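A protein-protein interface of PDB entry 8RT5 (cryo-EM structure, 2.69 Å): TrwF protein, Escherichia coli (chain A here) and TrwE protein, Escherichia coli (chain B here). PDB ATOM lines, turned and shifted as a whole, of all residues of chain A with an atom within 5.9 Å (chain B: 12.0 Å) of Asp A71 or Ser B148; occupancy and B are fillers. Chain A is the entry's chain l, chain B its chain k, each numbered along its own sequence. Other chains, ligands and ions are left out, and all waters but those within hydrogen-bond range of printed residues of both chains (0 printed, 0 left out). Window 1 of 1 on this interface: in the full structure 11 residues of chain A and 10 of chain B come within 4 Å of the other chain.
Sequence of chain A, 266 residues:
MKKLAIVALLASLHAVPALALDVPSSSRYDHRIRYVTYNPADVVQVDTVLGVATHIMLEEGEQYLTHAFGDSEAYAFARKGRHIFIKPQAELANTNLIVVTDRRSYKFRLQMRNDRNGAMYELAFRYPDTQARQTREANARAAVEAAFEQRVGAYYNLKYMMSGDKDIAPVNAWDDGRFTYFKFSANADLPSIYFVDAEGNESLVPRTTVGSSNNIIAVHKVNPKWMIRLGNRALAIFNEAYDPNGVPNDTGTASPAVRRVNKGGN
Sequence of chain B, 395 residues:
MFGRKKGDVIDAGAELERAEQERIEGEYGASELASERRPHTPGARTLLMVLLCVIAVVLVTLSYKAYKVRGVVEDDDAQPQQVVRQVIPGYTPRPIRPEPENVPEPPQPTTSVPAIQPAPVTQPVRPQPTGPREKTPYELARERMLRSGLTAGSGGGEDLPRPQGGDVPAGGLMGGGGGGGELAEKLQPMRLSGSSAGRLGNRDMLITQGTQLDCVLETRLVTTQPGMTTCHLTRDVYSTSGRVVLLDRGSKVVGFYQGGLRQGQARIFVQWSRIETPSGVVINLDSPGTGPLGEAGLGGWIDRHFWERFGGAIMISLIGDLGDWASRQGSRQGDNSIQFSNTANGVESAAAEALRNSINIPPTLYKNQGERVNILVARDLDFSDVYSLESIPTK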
ATOM      1  N   PHE A  69     -34.207   3.979 -15.856  1.00  0.00           N
ATOM      2  CA  PHE A  69     -33.249   4.513 -14.909  1.00  0.00           C
ATOM      3  C   PHE A  69     -33.881   5.654 -14.132  1.00  0.00           C
ATOM      4  O   PHE A  69     -34.654   6.448 -14.669  1.00  0.00           O
ATOM      5  CB  PHE A  69     -31.995   5.017 -15.620  1.00  0.00           C
ATOM      6  CG  PHE A  69     -31.009   3.947 -15.942  1.00  0.00           C
ATOM      7  CD1 PHE A  69     -30.139   3.482 -14.979  1.00  0.00           C
ATOM      8  CD2 PHE A  69     -30.938   3.417 -17.215  1.00  0.00           C
ATOM      9  CE1 PHE A  69     -29.227   2.504 -15.276  1.00  0.00           C
ATOM     10  CE2 PHE A  69     -30.027   2.443 -17.513  1.00  0.00           C
ATOM     11  CZ  PHE A  69     -29.170   1.986 -16.545  1.00  0.00           C
ATOM     12  N   GLY A  70     -33.548   5.726 -12.847  1.00  0.00           N
ATOM     13  CA  GLY A  70     -33.890   6.913 -12.088  1.00  0.00           C
ATOM     14  C   GLY A  70     -33.113   8.122 -12.563  1.00  0.00           C
ATOM     15  O   GLY A  70     -33.496   9.261 -12.297  1.00  0.00           O
ATOM     16  N   ASP A  71     -31.993   7.890 -13.244  1.00  0.00           N
ATOM     17  CA  ASP A  71     -31.195   8.933 -13.875  1.00  0.00           C
ATOM     18  C   ASP A  71     -30.489   8.313 -15.071  1.00  0.00           C
ATOM     19  O   ASP A  71     -29.498   7.600 -14.904  1.00  0.00           O
ATOM     20  CB  ASP A  71     -30.183   9.522 -12.888  1.00  0.00           C
ATOM     21  CG  ASP A  71     -29.362  10.647 -13.485  1.00  0.00           C
ATOM     22  OD1 ASP A  71     -28.549  11.229 -12.744  1.00  0.00           O
ATOM     23  OD2 ASP A  71     -29.533  10.972 -14.675  1.00  0.00           O
ATOM     24  N   SER A  72     -30.992   8.594 -16.275  1.00  0.00           N
ATOM     25  CA  SER A  72     -30.466   7.951 -17.474  1.00  0.00           C
ATOM     26  C   SER A  72     -29.054   8.392 -17.818  1.00  0.00           C
ATOM     27  O   SER A  72     -28.269   7.573 -18.300  1.00  0.00           O
ATOM     28  CB  SER A  72     -31.373   8.229 -18.668  1.00  0.00           C
ATOM     29  OG  SER A  72     -32.602   7.554 -18.530  1.00  0.00           O
ATOM     30  N   GLU A  73     -28.717   9.660 -17.605  1.00  0.00           N
ATOM     31  CA  GLU A  73     -27.398  10.161 -17.962  1.00  0.00           C
ATOM     32  C   GLU A  73     -26.309   9.730 -16.996  1.00  0.00           C
ATOM     33  O   GLU A  73     -25.130   9.964 -17.275  1.00  0.00           O
ATOM     34  CB  GLU A  73     -27.417  11.687 -18.053  1.00  0.00           C
ATOM     35  CG  GLU A  73     -28.652  12.235 -18.713  1.00  0.00           C
ATOM     36  CD  GLU A  73     -28.570  13.723 -18.958  1.00  0.00           C
ATOM     37  OE1 GLU A  73     -29.336  14.229 -19.804  1.00  0.00           O
ATOM     38  OE2 GLU A  73     -27.740  14.389 -18.306  1.00  0.00           O
ATOM     39  N   ALA A  74     -26.668   9.125 -15.870  1.00  0.00           N
ATOM     40  CA  ALA A  74     -25.660   8.649 -14.936  1.00  0.00           C
ATOM     41  C   ALA A  74     -25.011   7.354 -15.402  1.00  0.00           C
ATOM     42  O   ALA A  74     -23.854   7.093 -15.068  1.00  0.00           O
ATOM     43  CB  ALA A  74     -26.274   8.462 -13.552  1.00  0.00           C
ATOM     44  N   TYR A  75     -25.727   6.536 -16.165  1.00  0.00           N
ATOM     45  CA  TYR A  75     -25.251   5.222 -16.561  1.00  0.00           C
ATOM     46  C   TYR A  75     -25.464   5.007 -18.048  1.00  0.00           C
ATOM     47  O   TYR A  75     -26.349   5.607 -18.658  1.00  0.00           O
ATOM     48  CB  TYR A  75     -25.962   4.123 -15.782  1.00  0.00           C
ATOM     49  CG  TYR A  75     -25.477   4.007 -14.370  1.00  0.00           C
ATOM     50  CD1 TYR A  75     -25.986   4.821 -13.379  1.00  0.00           C
ATOM     51  CD2 TYR A  75     -24.505   3.089 -14.026  1.00  0.00           C
ATOM     52  CE1 TYR A  75     -25.543   4.726 -12.091  1.00  0.00           C
ATOM     53  CE2 TYR A  75     -24.055   2.988 -12.739  1.00  0.00           C
ATOM     54  CZ  TYR A  75     -24.579   3.810 -11.772  1.00  0.00           C
ATOM     55  OH  TYR A  75     -24.139   3.715 -10.478  1.00  0.00           O
ATOM     56  N   ASN A  94     -25.628   7.864  -8.504  1.00  0.00           N
ATOM     57  CA  ASN A  94     -26.397   7.100  -7.530  1.00  0.00           C
ATOM     58  C   ASN A  94     -27.861   7.159  -7.933  1.00  0.00           C
ATOM     59  O   ASN A  94     -28.504   8.203  -7.803  1.00  0.00           O
ATOM     60  CB  ASN A  94     -26.188   7.655  -6.126  1.00  0.00           C
ATOM     61  CG  ASN A  94     -24.761   7.534  -5.668  1.00  0.00           C
ATOM     62  OD1 ASN A  94     -23.922   8.375  -5.978  1.00  0.00           O
ATOM     63  ND2 ASN A  94     -24.473   6.486  -4.924  1.00  0.00           N
ATOM     64  N   THR A  95     -28.386   6.042  -8.422  1.00  0.00           N
ATOM     65  CA  THR A  95     -29.745   5.999  -8.944  1.00  0.00           C
ATOM     66  C   THR A  95     -30.277   4.582  -8.759  1.00  0.00           C
ATOM     67  O   THR A  95     -29.743   3.789  -7.979  1.00  0.00           O
ATOM     68  CB  THR A  95     -29.767   6.477 -10.403  1.00  0.00           C
ATOM     69  OG1 THR A  95     -31.118   6.591 -10.845  1.00  0.00           O
ATOM     70  CG2 THR A  95     -29.034   5.508 -11.302  1.00  0.00           C
ATOM     71  N   ASN A  96     -31.356   4.256  -9.461  1.00  0.00           N
ATOM     72  CA  ASN A  96     -31.910   2.914  -9.446  1.00  0.00           C
ATOM     73  C   ASN A  96     -32.188   2.474 -10.874  1.00  0.00           C
ATOM     74  O   ASN A  96     -32.316   3.295 -11.782  1.00  0.00           O
ATOM     75  CB  ASN A  96     -33.187   2.827  -8.597  1.00  0.00           C
ATOM     76  CG  ASN A  96     -34.386   3.481  -9.253  1.00  0.00           C
ATOM     77  OD1 ASN A  96     -34.279   4.544  -9.855  1.00  0.00           O
ATOM     78  ND2 ASN A  96     -35.537   2.842  -9.140  1.00  0.00           N
ATOM     79  N   PRO B 137     -20.605  19.454  -7.068  1.00  0.00           N
ATOM     80  CA  PRO B 137     -21.015  18.295  -7.866  1.00  0.00           C
ATOM     81  C   PRO B 137     -22.327  17.665  -7.430  1.00  0.00           C
ATOM     82  O   PRO B 137     -22.993  17.029  -8.256  1.00  0.00           O
ATOM     83  CB  PRO B 137     -19.803  17.358  -7.721  1.00  0.00           C
ATOM     84  CG  PRO B 137     -18.882  18.122  -6.702  1.00  0.00           C
ATOM     85  CD  PRO B 137     -19.819  18.909  -5.942  1.00  0.00           C
ATOM     86  N   TYR B 138     -22.731  17.827  -6.169  1.00  0.00           N
ATOM     87  CA  TYR B 138     -24.062  17.386  -5.767  1.00  0.00           C
ATOM     88  C   TYR B 138     -25.140  18.126  -6.550  1.00  0.00           C
ATOM     89  O   TYR B 138     -26.128  17.523  -6.983  1.00  0.00           O
ATOM     90  CB  TYR B 138     -24.252  17.590  -4.265  1.00  0.00           C
ATOM     91  CG  TYR B 138     -25.592  17.120  -3.749  1.00  0.00           C
ATOM     92  CD1 TYR B 138     -25.857  15.769  -3.577  1.00  0.00           C
ATOM     93  CD2 TYR B 138     -26.597  18.029  -3.441  1.00  0.00           C
ATOM     94  CE1 TYR B 138     -27.080  15.333  -3.108  1.00  0.00           C
ATOM     95  CE2 TYR B 138     -27.824  17.603  -2.972  1.00  0.00           C
ATOM     96  CZ  TYR B 138     -28.060  16.254  -2.808  1.00  0.00           C
ATOM     97  OH  TYR B 138     -29.280  15.824  -2.340  1.00  0.00           O
ATOM     98  N   GLU B 139     -24.961  19.432  -6.754  1.00  0.00           N
ATOM     99  CA  GLU B 139     -25.949  20.208  -7.496  1.00  0.00           C
ATOM    100  C   GLU B 139     -26.004  19.799  -8.962  1.00  0.00           C
ATOM    101  O   GLU B 139     -27.089  19.697  -9.546  1.00  0.00           O
ATOM    102  CB  GLU B 139     -25.649  21.700  -7.360  1.00  0.00           C
ATOM    103  CG  GLU B 139     -26.126  22.292  -6.046  1.00  0.00           C
ATOM    104  CD  GLU B 139     -25.742  23.748  -5.888  1.00  0.00           C
ATOM    105  OE1 GLU B 139     -25.724  24.233  -4.737  1.00  0.00           O
ATOM    106  OE2 GLU B 139     -25.456  24.406  -6.909  1.00  0.00           O
ATOM    107  N   LEU B 140     -24.844  19.575  -9.581  1.00  0.00           N
ATOM    108  CA  LEU B 140     -24.831  19.122 -10.968  1.00  0.00           C
ATOM    109  C   LEU B 140     -25.449  17.738 -11.097  1.00  0.00           C
ATOM    110  O   LEU B 140     -26.163  17.455 -12.065  1.00  0.00           O
ATOM    111  CB  LEU B 140     -23.403  19.127 -11.507  1.00  0.00           C
ATOM    112  CG  LEU B 140     -22.740  20.496 -11.637  1.00  0.00           C
ATOM    113  CD1 LEU B 140     -21.289  20.344 -12.044  1.00  0.00           C
ATOM    114  CD2 LEU B 140     -23.488  21.333 -12.651  1.00  0.00           C
ATOM    115  N   ALA B 141     -25.195  16.863 -10.123  1.00  0.00           N
ATOM    116  CA  ALA B 141     -25.827  15.551 -10.122  1.00  0.00           C
ATOM    117  C   ALA B 141     -27.338  15.671 -10.005  1.00  0.00           C
ATOM    118  O   ALA B 141     -28.079  14.945 -10.672  1.00  0.00           O
ATOM    119  CB  ALA B 141     -25.270  14.705  -8.978  1.00  0.00           C
ATOM    120  N   ARG B 142     -27.809  16.574  -9.145  1.00  0.00           N
ATOM    121  CA  ARG B 142     -29.243  16.740  -8.940  1.00  0.00           C
ATOM    122  C   ARG B 142     -29.908  17.290 -10.197  1.00  0.00           C
ATOM    123  O   ARG B 142     -31.001  16.850 -10.581  1.00  0.00           O
ATOM    124  CB  ARG B 142     -29.462  17.649  -7.730  1.00  0.00           C
ATOM    125  CG  ARG B 142     -30.877  18.094  -7.440  1.00  0.00           C
ATOM    126  CD  ARG B 142     -30.846  19.078  -6.285  1.00  0.00           C
ATOM    127  NE  ARG B 142     -32.168  19.542  -5.877  1.00  0.00           N
ATOM    128  CZ  ARG B 142     -32.980  18.849  -5.085  1.00  0.00           C
ATOM    129  NH1 ARG B 142     -32.594  17.683  -4.594  1.00  0.00           N
ATOM    130  NH2 ARG B 142     -34.166  19.336  -4.757  1.00  0.00           N
ATOM    131  N   GLU B 143     -29.248  18.241 -10.861  1.00  0.00           N
ATOM    132  CA  GLU B 143     -29.742  18.742 -12.139  1.00  0.00           C
ATOM    133  C   GLU B 143     -29.768  17.645 -13.195  1.00  0.00           C
ATOM    134  O   GLU B 143     -30.705  17.569 -13.997  1.00  0.00           O
ATOM    135  CB  GLU B 143     -28.885  19.917 -12.604  1.00  0.00           C
ATOM    136  CG  GLU B 143     -29.321  20.527 -13.926  1.00  0.00           C
ATOM    137  CD  GLU B 143     -30.233  21.724 -13.755  1.00  0.00           C
ATOM    138  OE1 GLU B 143     -30.262  22.299 -12.648  1.00  0.00           O
ATOM    139  OE2 GLU B 143     -30.920  22.090 -14.733  1.00  0.00           O
ATOM    140  N   ARG B 144     -28.741  16.791 -13.222  1.00  0.00           N
ATOM    141  CA  ARG B 144     -28.738  15.670 -14.156  1.00  0.00           C
ATOM    142  C   ARG B 144     -29.884  14.710 -13.874  1.00  0.00           C
ATOM    143  O   ARG B 144     -30.556  14.243 -14.800  1.00  0.00           O
ATOM    144  CB  ARG B 144     -27.399  14.938 -14.092  1.00  0.00           C
ATOM    145  CG  ARG B 144     -27.430  13.550 -14.706  1.00  0.00           C
ATOM    146  CD  ARG B 144     -26.059  12.936 -14.793  1.00  0.00           C
ATOM    147  NE  ARG B 144     -25.286  13.100 -13.566  1.00  0.00           N
ATOM    148  CZ  ARG B 144     -25.432  12.352 -12.480  1.00  0.00           C
ATOM    149  NH1 ARG B 144     -24.671  12.568 -11.420  1.00  0.00           N
ATOM    150  NH2 ARG B 144     -26.339  11.394 -12.447  1.00  0.00           N
ATOM    151  N   MET B 145     -30.125  14.405 -12.597  1.00  0.00           N
ATOM    152  CA  MET B 145     -31.207  13.494 -12.243  1.00  0.00           C
ATOM    153  C   MET B 145     -32.560  14.059 -12.644  1.00  0.00           C
ATOM    154  O   MET B 145     -33.410  13.331 -13.163  1.00  0.00           O
ATOM    155  CB  MET B 145     -31.167  13.172 -10.750  1.00  0.00           C
ATOM    156  CG  MET B 145     -29.994  12.302 -10.351  1.00  0.00           C
ATOM    157  SD  MET B 145     -29.957  11.818  -8.620  1.00  0.00           S
ATOM    158  CE  MET B 145     -29.243  13.275  -7.882  1.00  0.00           C
ATOM    159  N   LEU B 146     -32.782  15.354 -12.420  1.00  0.00           N
ATOM    160  CA  LEU B 146     -34.020  15.970 -12.891  1.00  0.00           C
ATOM    161  C   LEU B 146     -34.117  15.949 -14.412  1.00  0.00           C
ATOM    162  O   LEU B 146     -35.198  15.731 -14.966  1.00  0.00           O
ATOM    163  CB  LEU B 146     -34.134  17.397 -12.363  1.00  0.00           C
ATOM    164  CG  LEU B 146     -34.318  17.531 -10.857  1.00  0.00           C
ATOM    165  CD1 LEU B 146     -34.652  18.954 -10.502  1.00  0.00           C
ATOM    166  CD2 LEU B 146     -35.452  16.628 -10.438  1.00  0.00           C
ATOM    167  N   ARG B 147     -33.002  16.172 -15.100  1.00  0.00           N
ATOM    168  CA  ARG B 147     -33.040  16.389 -16.543  1.00  0.00           C
ATOM    169  C   ARG B 147     -33.307  15.105 -17.324  1.00  0.00           C
ATOM    170  O   ARG B 147     -33.999  15.131 -18.347  1.00  0.00           O
ATOM    171  CB  ARG B 147     -31.726  17.035 -16.979  1.00  0.00           C
ATOM    172  CG  ARG B 147     -31.648  17.438 -18.426  1.00  0.00           C
ATOM    173  CD  ARG B 147     -30.325  18.127 -18.695  1.00  0.00           C
ATOM    174  NE  ARG B 147     -29.183  17.242 -18.509  1.00  0.00           N
ATOM    175  CZ  ARG B 147     -28.276  17.396 -17.549  1.00  0.00           C
ATOM    176  NH1 ARG B 147     -28.384  18.397 -16.690  1.00  0.00           N
ATOM    177  NH2 ARG B 147     -27.264  16.549 -17.448  1.00  0.00           N
ATOM    178  N   SER B 148     -32.772  13.978 -16.865  1.00  0.00           N
ATOM    179  CA  SER B 148     -32.736  12.770 -17.680  1.00  0.00           C
ATOM    180  C   SER B 148     -34.101  12.093 -17.784  1.00  0.00           C
ATOM    181  O   SER B 148     -34.955  12.216 -16.904  1.00  0.00           O
ATOM    182  CB  SER B 148     -31.723  11.783 -17.111  1.00  0.00           C
ATOM    183  OG  SER B 148     -31.811  11.716 -15.703  1.00  0.00           O
ATOM    184  N   GLY B 149     -34.292  11.366 -18.885  1.00  0.00           N
ATOM    185  CA  GLY B 149     -35.461  10.537 -19.069  1.00  0.00           C
ATOM    186  C   GLY B 149     -35.311   9.167 -18.432  1.00  0.00           C
ATOM    187  O   GLY B 149     -34.326   8.854 -17.765  1.00  0.00           O
ATOM    188  N   LEU B 150     -36.334   8.336 -18.632  1.00  0.00           N
ATOM    189  CA  LEU B 150     -36.289   6.966 -18.126  1.00  0.00           C
ATOM    190  C   LEU B 150     -35.405   6.067 -18.979  1.00  0.00           C
ATOM    191  O   LEU B 150     -34.771   5.142 -18.462  1.00  0.00           O
ATOM    192  CB  LEU B 150     -37.703   6.406 -18.020  1.00  0.00           C
ATOM    193  CG  LEU B 150     -38.652   7.372 -17.332  1.00  0.00           C
ATOM    194  CD1 LEU B 150     -40.077   7.092 -17.634  1.00  0.00           C
ATOM    195  CD2 LEU B 150     -38.426   7.103 -15.885  1.00  0.00           C
ATOM    196  N   THR B 151     -35.345   6.317 -20.280  1.00  0.00           N
ATOM    197  CA  THR B 151     -34.511   5.537 -21.180  1.00  0.00           C
ATOM    198  C   THR B 151     -33.665   6.501 -21.993  1.00  0.00           C
ATOM    199  O   THR B 151     -34.138   7.576 -22.371  1.00  0.00           O
ATOM    200  CB  THR B 151     -35.369   4.645 -22.091  1.00  0.00           C
ATOM    201  OG1 THR B 151     -35.965   3.603 -21.310  1.00  0.00           O
ATOM    202  CG2 THR B 151     -34.543   4.017 -23.197  1.00  0.00           C
ATOM    203  N   ALA B 152     -32.414   6.130 -22.240  1.00  0.00           N
ATOM    204  CA  ALA B 152     -31.536   6.940 -23.067  1.00  0.00           C
ATOM    205  C   ALA B 152     -31.899   6.760 -24.535  1.00  0.00           C
ATOM    206  O   ALA B 152     -32.114   5.637 -24.999  1.00  0.00           O
ATOM    207  CB  ALA B 152     -30.077   6.562 -22.828  1.00  0.00           C
ATOM    208  N   GLY B 153     -31.971   7.868 -25.261  1.00  0.00           N
ATOM    209  CA  GLY B 153     -32.318   7.827 -26.668  1.00  0.00           C
ATOM    210  C   GLY B 153     -32.524   9.201 -27.273  1.00  0.00           C
ATOM    211  O   GLY B 153     -31.665   9.706 -27.994  1.00  0.00           O
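Of the 17 printed residues of chain B, 8 touch a printed residue of chain A. Hydrophobic or aromatic side chains of chain B that line the printed part of chain A: Met B145. Along chain B the printed residues that touch a printed residue of chain A span positions 144 to 152. Of the 10 printed residues of chain A, 6 touch a printed residue of chain B. Hydrophobic or aromatic side chains of chain A that line the printed part of chain B: Phe A69 and Ala A74. Among the printed residues, Asp or Glu carboxylates within 4 Å of a Lys or Arg side-chain nitrogen of the other chain: Asp A71 with Arg B144 (2.2 Å) and Glu A73 with Arg B147 (2.4 Å).
Phe A69 touches just these residues of chain B: Gly B149 (3.9 Å) and Leu B150 (2.9 Å). No residue of chain B comes within 4 Å of Gly A70. Asp A71 touches three residues of chain B. Of the printed residues of chain B, Ser A72 touches Ser B148, Gly B149, Leu B150, Thr B151 and Ala B152. Of the printed residues of chain B, Glu A73 touches Arg B144, Arg B147 and Ser B148. Of the printed residues of chain B, Asn A94 touches Met B145 (3.98 Å). No residue of chain B comes within 4 Å of Thr A95. Asn A96 touches none of the printed residues of chain B. Pro B137 touches none of the printed residues of chain A. Arg B142 touches none of the printed residues of chain A. Ser B148 touches just these residues of chain A: Asp A71 (2.6 Å), Ser A72 (3.3 Å) and Glu A73 (3.5 Å). Of the printed residues of chain A, Leu B150 touches Phe A69 (2.9 Å) and Ser A72 (3.2 Å). The nearest residue of chain A that does not touch Ser B148 is Gly A70 (4.5 Å). The nearest printed residue of chain B that does not touch Asn A94 is Arg B144 (5.3 Å).
The side-chain hydroxyl (OG) of Ser B148 sits at hydrogen-bond distance from the backbone carbonyl oxygen (O) of Arg B144 (3.0 Å). OD2 of Asp A71 lies within hydrogen-bond range of N of Glu A73 (3.3 Å). O of Met B145 lies within hydrogen-bond range of OG of Ser B148, 3.4 Å away. The backbone NH (N) of Asp A71 sits at hydrogen-bond distance from the side-chain hydroxyl (OG1) of Thr A95 (2.9 Å).
Phe A69 touches Gly B149 (O to O, 3.9 Å). Asp A71 touches Met B145 (OD1 to CG, 3.0 Å). N of Ala B152 touches OG of Ser A72, 3.98 Å away. Glu A73 touches Arg B144. CG of Glu A73 touches CB of Ser B148, 3.5 Å away. Arg B144 touches Ala A74. Asn A94 touches Met B145.
OG of Ser A72 lies close to O of Gly B149, 2.3 Å away. The backbone NH of Ser A72 lies within hydrogen-bond range of the side-chain hydroxyl of Ser B148, at 3.3 Å. The backbone carbonyl oxygen (O) of Leu B150 sits close to the side-chain hydroxyl (OG) of Ser A72 (3.2 Å). NE of Arg B147 is in salt-bridge range of OE2 of Glu A73. OG of Ser B148 is in hydrogen-bond range of OD2 of Asp A71 (2.6 Å). The side-chain carboxylate (OD1) of Asp A71 lies within salt-bridge range of the guanidinium group (NE) of Arg B144, 3.9 Å away. The backbone carbonyl oxygen (O) of Leu B150 is in hydrogen-bond range of the backbone NH (N) of Phe A69 (2.9 Å). N of Thr B151 is in hydrogen-bond range of OG of Ser A72 (3.5 Å).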
